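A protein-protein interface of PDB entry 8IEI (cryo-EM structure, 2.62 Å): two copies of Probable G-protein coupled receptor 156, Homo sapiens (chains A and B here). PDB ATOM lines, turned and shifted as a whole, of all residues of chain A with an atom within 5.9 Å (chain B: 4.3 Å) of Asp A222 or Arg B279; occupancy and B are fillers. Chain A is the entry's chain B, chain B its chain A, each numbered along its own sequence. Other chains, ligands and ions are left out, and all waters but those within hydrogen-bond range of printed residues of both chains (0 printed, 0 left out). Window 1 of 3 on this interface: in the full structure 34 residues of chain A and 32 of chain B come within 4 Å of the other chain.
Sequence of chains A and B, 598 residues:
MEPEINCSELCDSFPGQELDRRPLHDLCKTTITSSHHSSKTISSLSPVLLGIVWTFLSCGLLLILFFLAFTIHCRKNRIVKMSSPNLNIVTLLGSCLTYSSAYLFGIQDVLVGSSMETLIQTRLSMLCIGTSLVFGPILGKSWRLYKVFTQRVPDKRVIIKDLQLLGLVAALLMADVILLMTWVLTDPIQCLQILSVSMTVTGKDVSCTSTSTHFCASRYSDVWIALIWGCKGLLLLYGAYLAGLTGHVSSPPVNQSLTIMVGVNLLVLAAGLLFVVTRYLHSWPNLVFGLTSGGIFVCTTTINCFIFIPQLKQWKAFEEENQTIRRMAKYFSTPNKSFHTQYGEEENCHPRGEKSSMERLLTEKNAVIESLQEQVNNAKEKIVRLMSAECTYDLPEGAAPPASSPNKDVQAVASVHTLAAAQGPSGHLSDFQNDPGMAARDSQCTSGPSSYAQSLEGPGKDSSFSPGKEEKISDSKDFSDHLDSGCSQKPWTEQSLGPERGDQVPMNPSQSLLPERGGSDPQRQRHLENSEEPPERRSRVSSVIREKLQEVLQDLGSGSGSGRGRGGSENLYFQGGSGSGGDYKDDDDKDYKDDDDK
The side-chain carboxylate (OD2) of Asp B222 is in salt-bridge range of the guanidinium group (NH1) of Arg A279 (3.4 Å).
The side-chain carboxylate (OD2) of Asp A222 is in salt-bridge range of the guanidinium group (NH1) of Arg B279, at 2.6 Å.
The backbone NH (N) of Ser A221 sits at hydrogen-bond distance from the side-chain hydroxyl (OH) of Tyr B280, at 3.4 Å.
OH of Tyr B280 sits at hydrogen-bond distance from N of Asp A222 (3.0 Å).
NH2 of Arg B279 lies within salt-bridge range of OD1 of Asp B222, at 3.0 Å.
A ring nitrogen (ND1) of His B282 lies within hydrogen-bond range of the backbone carbonyl oxygen (O) of Tyr B280 (3.4 Å).
The indole nitrogen (NE1) of Trp A224 lies close to the backbone carbonyl oxygen (O) of Tyr A220, at 3.4 Å.
OD1 of Asp A222 lies within salt-bridge range of NH2 of Arg A279 (2.5 Å).
C of Tyr A220 touches OH of Tyr B280, at 3.4 Å.
CG1 of Val B276 touches CG2 of Val A223, 3.9 Å away.
Val A223 touches Tyr B280.
Val B276 touches Ala A226.
NH1 of Arg A279 touches NH1 of Arg B279, 3.998 Å away.
Of the printed residues of chain B, Tyr A220 touches Tyr B280 (3.4 Å).
Printed residues of chain B within 4 Å of Ser A221: Tyr B280 (3.4 Å).
Asp A222 touches two residues of chain B.
Of the printed residues of chain B, Val A223 touches Val B276 and Tyr B280.
Ile A225 touches none of the printed residues of chain B.
Printed residues of chain B within 4 Å of Ala A226: Val B276 (3.2 Å).
Of the printed residues of chain A, Asp B222 touches Arg A279.
Of the printed residues of chain A, Arg B279 touches Asp A222 and Arg A279.
The nearest printed residue of chain A that does not touch Arg B279 is Phe A275 (6.2 Å).
The nearest printed residue of chain B that does not touch Arg A279 is Phe B275 (6.3 Å).
Of the 10 printed residues of chain A, 6 touch a printed residue of chain B.
Printed residues of chain A that touch a printed residue of chain B: Tyr A220, Ser A221, Asp A222, Val A223, Ala A226 and Arg A279.
Hydrophobic or aromatic side chains of chain A within 4 Å of the printed part of chain B: Tyr A220, Val A223 and Ala A226.
Hydrophobic or aromatic side chains of chain B within 4 Å of the printed part of chain A: Val B276 and Tyr B280.
Among the printed residues, 9 pairs touch across the chains.
Among the printed residues, Asp or Glu carboxylates within 4 Å of a Lys or Arg side-chain nitrogen of the other chain: Asp A222 with Arg B279 (2.6 Å) and Arg A279 with Asp B222 (3.4 Å).
Asp A222 touches Arg B279, and with the chains exchanged Arg A279 touches Asp B222.
Arg A279 touches its own counterpart, Arg B279.
Of the 9 pairs that touch across the chains among the printed residues, 3 have their exchanged pair printed and touching as well.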
ATOM      1  N   TYR A 220      19.870  10.059   9.008  1.00  0.00           N
ATOM      2  CA  TYR A 220      19.991   9.377  10.292  1.00  0.00           C
ATOM      3  C   TYR A 220      18.813   9.753  11.182  1.00  0.00           C
ATOM      4  O   TYR A 220      18.999  10.141  12.337  1.00  0.00           O
ATOM      5  CB  TYR A 220      21.312   9.738  10.969  1.00  0.00           C
ATOM      6  CG  TYR A 220      22.516   9.134  10.293  1.00  0.00           C
ATOM      7  CD1 TYR A 220      22.904   7.832  10.559  1.00  0.00           C
ATOM      8  CD2 TYR A 220      23.272   9.872   9.394  1.00  0.00           C
ATOM      9  CE1 TYR A 220      24.004   7.278   9.942  1.00  0.00           C
ATOM     10  CE2 TYR A 220      24.372   9.329   8.774  1.00  0.00           C
ATOM     11  CZ  TYR A 220      24.734   8.032   9.051  1.00  0.00           C
ATOM     12  OH  TYR A 220      25.835   7.487   8.434  1.00  0.00           O
ATOM     13  N   SER A 221      17.599   9.655  10.638  1.00  0.00           N
ATOM     14  CA  SER A 221      16.418  10.173  11.325  1.00  0.00           C
ATOM     15  C   SER A 221      16.192   9.489  12.669  1.00  0.00           C
ATOM     16  O   SER A 221      15.798  10.141  13.644  1.00  0.00           O
ATOM     17  CB  SER A 221      15.189  10.001  10.438  1.00  0.00           C
ATOM     18  OG  SER A 221      14.987   8.638  10.114  1.00  0.00           O
ATOM     19  N   ASP A 222      16.416   8.176  12.737  1.00  0.00           N
ATOM     20  CA  ASP A 222      16.184   7.457  13.984  1.00  0.00           C
ATOM     21  C   ASP A 222      17.128   7.909  15.092  1.00  0.00           C
ATOM     22  O   ASP A 222      16.779   7.799  16.266  1.00  0.00           O
ATOM     23  CB  ASP A 222      16.308   5.951  13.758  1.00  0.00           C
ATOM     24  CG  ASP A 222      15.097   5.360  13.074  1.00  0.00           C
ATOM     25  OD1 ASP A 222      13.964   5.747  13.421  1.00  0.00           O
ATOM     26  OD2 ASP A 222      15.277   4.510  12.181  1.00  0.00           O
ATOM     27  N   VAL A 223      18.310   8.431  14.756  1.00  0.00           N
ATOM     28  CA  VAL A 223      19.201   8.947  15.795  1.00  0.00           C
ATOM     29  C   VAL A 223      18.570  10.155  16.474  1.00  0.00           C
ATOM     30  O   VAL A 223      18.528  10.253  17.708  1.00  0.00           O
ATOM     31  CB  VAL A 223      20.580   9.289  15.203  1.00  0.00           C
ATOM     32  CG1 VAL A 223      21.525   9.777  16.294  1.00  0.00           C
ATOM     33  CG2 VAL A 223      21.158   8.077  14.493  1.00  0.00           C
ATOM     34  N   TRP A 224      18.039  11.080  15.674  1.00  0.00           N
ATOM     35  CA  TRP A 224      17.414  12.274  16.233  1.00  0.00           C
ATOM     36  C   TRP A 224      16.128  11.917  16.968  1.00  0.00           C
ATOM     37  O   TRP A 224      15.811  12.505  18.007  1.00  0.00           O
ATOM     38  CB  TRP A 224      17.155  13.288  15.120  1.00  0.00           C
ATOM     39  CG  TRP A 224      18.340  13.519  14.241  1.00  0.00           C
ATOM     40  CD1 TRP A 224      18.470  13.136  12.943  1.00  0.00           C
ATOM     41  CD2 TRP A 224      19.556  14.192  14.587  1.00  0.00           C
ATOM     42  NE1 TRP A 224      19.692  13.516  12.459  1.00  0.00           N
ATOM     43  CE2 TRP A 224      20.378  14.171  13.446  1.00  0.00           C
ATOM     44  CE3 TRP A 224      20.029  14.809  15.749  1.00  0.00           C
ATOM     45  CZ2 TRP A 224      21.646  14.740  13.433  1.00  0.00           C
ATOM     46  CZ3 TRP A 224      21.288  15.373  15.732  1.00  0.00           C
ATOM     47  CH2 TRP A 224      22.082  15.335  14.582  1.00  0.00           C
ATOM     48  N   ILE A 225      15.385  10.940  16.443  1.00  0.00           N
ATOM     49  CA  ILE A 225      14.190  10.436  17.117  1.00  0.00           C
ATOM     50  C   ILE A 225      14.543   9.861  18.478  1.00  0.00           C
ATOM     51  O   ILE A 225      13.960  10.229  19.507  1.00  0.00           O
ATOM     52  CB  ILE A 225      13.495   9.389  16.226  1.00  0.00           C
ATOM     53  CG1 ILE A 225      12.821  10.097  15.047  1.00  0.00           C
ATOM     54  CG2 ILE A 225      12.545   8.474  17.009  1.00  0.00           C
ATOM     55  CD1 ILE A 225      12.675   9.233  13.837  1.00  0.00           C
ATOM     56  N   ALA A 226      15.516   8.958  18.513  1.00  0.00           N
ATOM     57  CA  ALA A 226      15.895   8.371  19.784  1.00  0.00           C
ATOM     58  C   ALA A 226      16.364   9.443  20.750  1.00  0.00           C
ATOM     59  O   ALA A 226      16.041   9.389  21.934  1.00  0.00           O
ATOM     60  CB  ALA A 226      16.975   7.317  19.579  1.00  0.00           C
ATOM     61  N   LEU A 227      17.073  10.458  20.254  1.00  0.00           N
ATOM     62  CA  LEU A 227      17.546  11.524  21.133  1.00  0.00           C
ATOM     63  C   LEU A 227      16.393  12.325  21.738  1.00  0.00           C
ATOM     64  O   LEU A 227      16.386  12.598  22.943  1.00  0.00           O
ATOM     65  CB  LEU A 227      18.497  12.442  20.365  1.00  0.00           C
ATOM     66  CG  LEU A 227      19.986  12.097  20.447  1.00  0.00           C
ATOM     67  CD1 LEU A 227      20.769  12.989  19.505  1.00  0.00           C
ATOM     68  CD2 LEU A 227      20.525  12.229  21.866  1.00  0.00           C
ATOM     69  N   PHE A 275       4.327   8.072  15.577  1.00  0.00           N
ATOM     70  CA  PHE A 275       5.572   7.624  14.962  1.00  0.00           C
ATOM     71  C   PHE A 275       5.328   6.432  14.043  1.00  0.00           C
ATOM     72  O   PHE A 275       5.753   6.432  12.881  1.00  0.00           O
ATOM     73  CB  PHE A 275       6.573   7.269  16.064  1.00  0.00           C
ATOM     74  CG  PHE A 275       7.809   6.566  15.575  1.00  0.00           C
ATOM     75  CD1 PHE A 275       8.657   7.167  14.662  1.00  0.00           C
ATOM     76  CD2 PHE A 275       8.123   5.297  16.036  1.00  0.00           C
ATOM     77  CE1 PHE A 275       9.789   6.517  14.221  1.00  0.00           C
ATOM     78  CE2 PHE A 275       9.252   4.646  15.593  1.00  0.00           C
ATOM     79  CZ  PHE A 275      10.086   5.257  14.687  1.00  0.00           C
ATOM     80  N   ARG A 279       5.419   6.384   9.940  1.00  0.00           N
ATOM     81  CA  ARG A 279       6.449   5.581   9.292  1.00  0.00           C
ATOM     82  C   ARG A 279       5.854   4.618   8.273  1.00  0.00           C
ATOM     83  O   ARG A 279       6.372   4.497   7.157  1.00  0.00           O
ATOM     84  CB  ARG A 279       7.249   4.819  10.344  1.00  0.00           C
ATOM     85  CG  ARG A 279       8.429   4.044   9.790  1.00  0.00           C
ATOM     86  CD  ARG A 279       9.235   3.439  10.911  1.00  0.00           C
ATOM     87  NE  ARG A 279      10.142   4.422  11.493  1.00  0.00           N
ATOM     88  CZ  ARG A 279      11.422   4.575  11.176  1.00  0.00           C
ATOM     89  NH1 ARG A 279      12.026   3.790  10.297  1.00  0.00           N
ATOM     90  NH2 ARG A 279      12.119   5.547  11.757  1.00  0.00           N
ATOM     91  N   ASP B 222       9.441  -1.699  13.510  1.00  0.00           N
ATOM     92  CA  ASP B 222       9.248  -0.517  14.332  1.00  0.00           C
ATOM     93  C   ASP B 222       7.919  -0.536  15.071  1.00  0.00           C
ATOM     94  O   ASP B 222       7.826   0.057  16.145  1.00  0.00           O
ATOM     95  CB  ASP B 222       9.351   0.740  13.471  1.00  0.00           C
ATOM     96  CG  ASP B 222      10.765   1.008  13.009  1.00  0.00           C
ATOM     97  OD1 ASP B 222      11.616   1.338  13.858  1.00  0.00           O
ATOM     98  OD2 ASP B 222      11.032   0.879  11.798  1.00  0.00           O
ATOM     99  N   ILE B 225       8.664  -2.697  18.067  1.00  0.00           N
ATOM    100  CA  ILE B 225       9.513  -1.876  18.925  1.00  0.00           C
ATOM    101  C   ILE B 225       8.670  -0.857  19.678  1.00  0.00           C
ATOM    102  O   ILE B 225       8.793  -0.706  20.897  1.00  0.00           O
ATOM    103  CB  ILE B 225      10.613  -1.197  18.083  1.00  0.00           C
ATOM    104  CG1 ILE B 225      11.656  -2.226  17.643  1.00  0.00           C
ATOM    105  CG2 ILE B 225      11.264  -0.034  18.837  1.00  0.00           C
ATOM    106  CD1 ILE B 225      12.551  -1.754  16.518  1.00  0.00           C
ATOM    107  N   PHE B 275      19.275   0.696  20.815  1.00  0.00           N
ATOM    108  CA  PHE B 275      18.410   0.772  19.645  1.00  0.00           C
ATOM    109  C   PHE B 275      19.109   1.500  18.505  1.00  0.00           C
ATOM    110  O   PHE B 275      19.182   0.991  17.380  1.00  0.00           O
ATOM    111  CB  PHE B 275      17.101   1.473  20.017  1.00  0.00           C
ATOM    112  CG  PHE B 275      16.264   1.882  18.834  1.00  0.00           C
ATOM    113  CD1 PHE B 275      15.630   0.934  18.051  1.00  0.00           C
ATOM    114  CD2 PHE B 275      16.114   3.217  18.506  1.00  0.00           C
ATOM    115  CE1 PHE B 275      14.864   1.312  16.966  1.00  0.00           C
ATOM    116  CE2 PHE B 275      15.350   3.596  17.422  1.00  0.00           C
ATOM    117  CZ  PHE B 275      14.725   2.641  16.654  1.00  0.00           C
ATOM    118  N   VAL B 276      19.665   2.682  18.788  1.00  0.00           N
ATOM    119  CA  VAL B 276      20.326   3.453  17.736  1.00  0.00           C
ATOM    120  C   VAL B 276      21.537   2.697  17.196  1.00  0.00           C
ATOM    121  O   VAL B 276      21.742   2.598  15.978  1.00  0.00           O
ATOM    122  CB  VAL B 276      20.719   4.845  18.263  1.00  0.00           C
ATOM    123  CG1 VAL B 276      21.745   5.512  17.353  1.00  0.00           C
ATOM    124  CG2 VAL B 276      19.496   5.712  18.391  1.00  0.00           C
ATOM    125  N   VAL B 277      22.360   2.152  18.097  1.00  0.00           N
ATOM    126  CA  VAL B 277      23.604   1.516  17.682  1.00  0.00           C
ATOM    127  C   VAL B 277      23.319   0.281  16.836  1.00  0.00           C
ATOM    128  O   VAL B 277      23.960   0.064  15.803  1.00  0.00           O
ATOM    129  CB  VAL B 277      24.459   1.185  18.918  1.00  0.00           C
ATOM    130  CG1 VAL B 277      25.545   0.169  18.587  1.00  0.00           C
ATOM    131  CG2 VAL B 277      25.073   2.455  19.481  1.00  0.00           C
ATOM    132  N   THR B 278      22.362  -0.549  17.255  1.00  0.00           N
ATOM    133  CA  THR B 278      22.000  -1.706  16.450  1.00  0.00           C
ATOM    134  C   THR B 278      21.390  -1.289  15.120  1.00  0.00           C
ATOM    135  O   THR B 278      21.639  -1.936  14.099  1.00  0.00           O
ATOM    136  CB  THR B 278      21.024  -2.596  17.218  1.00  0.00           C
ATOM    137  OG1 THR B 278      21.443  -2.698  18.584  1.00  0.00           O
ATOM    138  CG2 THR B 278      20.972  -3.982  16.605  1.00  0.00           C
ATOM    139  N   ARG B 279      20.589  -0.219  15.109  1.00  0.00           N
ATOM    140  CA  ARG B 279      19.964   0.217  13.868  1.00  0.00           C
ATOM    141  C   ARG B 279      21.004   0.649  12.844  1.00  0.00           C
ATOM    142  O   ARG B 279      20.923   0.258  11.674  1.00  0.00           O
ATOM    143  CB  ARG B 279      18.981   1.353  14.166  1.00  0.00           C
ATOM    144  CG  ARG B 279      18.302   1.994  12.955  1.00  0.00           C
ATOM    145  CD  ARG B 279      17.508   0.997  12.136  1.00  0.00           C
ATOM    146  NE  ARG B 279      16.449   0.364  12.915  1.00  0.00           N
ATOM    147  CZ  ARG B 279      15.212   0.826  13.048  1.00  0.00           C
ATOM    148  NH1 ARG B 279      14.826   1.960  12.487  1.00  0.00           N
ATOM    149  NH2 ARG B 279      14.337   0.130  13.767  1.00  0.00           N
ATOM    150  N   TYR B 280      21.997   1.435  13.262  1.00  0.00           N
ATOM    151  CA  TYR B 280      22.905   2.084  12.320  1.00  0.00           C
ATOM    152  C   TYR B 280      24.293   1.461  12.262  1.00  0.00           C
ATOM    153  O   TYR B 280      24.841   1.307  11.167  1.00  0.00           O
ATOM    154  CB  TYR B 280      23.027   3.569  12.659  1.00  0.00           C
ATOM    155  CG  TYR B 280      21.787   4.335  12.287  1.00  0.00           C
ATOM    156  CD1 TYR B 280      21.476   4.576  10.958  1.00  0.00           C
ATOM    157  CD2 TYR B 280      20.911   4.789  13.255  1.00  0.00           C
ATOM    158  CE1 TYR B 280      20.340   5.258  10.608  1.00  0.00           C
ATOM    159  CE2 TYR B 280      19.774   5.470  12.914  1.00  0.00           C
ATOM    160  CZ  TYR B 280      19.490   5.705  11.588  1.00  0.00           C
ATOM    161  OH  TYR B 280      18.356   6.390  11.229  1.00  0.00           O
ATOM    162  N   LEU B 281      24.882   1.103  13.398  1.00  0.00           N
ATOM    163  CA  LEU B 281      26.234   0.544  13.413  1.00  0.00           C
ATOM    164  C   LEU B 281      26.204  -0.980  13.333  1.00  0.00           C
ATOM    165  O   LEU B 281      26.807  -1.680  14.142  1.00  0.00           O
ATOM    166  CB  LEU B 281      26.977   1.020  14.656  1.00  0.00           C
ATOM    167  CG  LEU B 281      27.515   2.453  14.614  1.00  0.00           C
ATOM    168  CD1 LEU B 281      26.398   3.477  14.714  1.00  0.00           C
ATOM    169  CD2 LEU B 281      28.526   2.658  15.722  1.00  0.00           C
ATOM    170  N   HIS B 282      25.494  -1.510  12.339  1.00  0.00           N
ATOM    171  CA  HIS B 282      25.433  -2.955  12.149  1.00  0.00           C
ATOM    172  C   HIS B 282      26.694  -3.520  11.509  1.00  0.00           C
ATOM    173  O   HIS B 282      26.898  -4.738  11.561  1.00  0.00           O
ATOM    174  CB  HIS B 282      24.216  -3.341  11.298  1.00  0.00           C
ATOM    175  CG  HIS B 282      24.169  -2.674   9.959  1.00  0.00           C
ATOM    176  ND1 HIS B 282      23.536  -1.467   9.752  1.00  0.00           N
ATOM    177  CD2 HIS B 282      24.674  -3.043   8.759  1.00  0.00           C
ATOM    178  CE1 HIS B 282      23.653  -1.122   8.482  1.00  0.00           C
ATOM    179  NE2 HIS B 282      24.340  -2.060   7.858  1.00  0.00           N
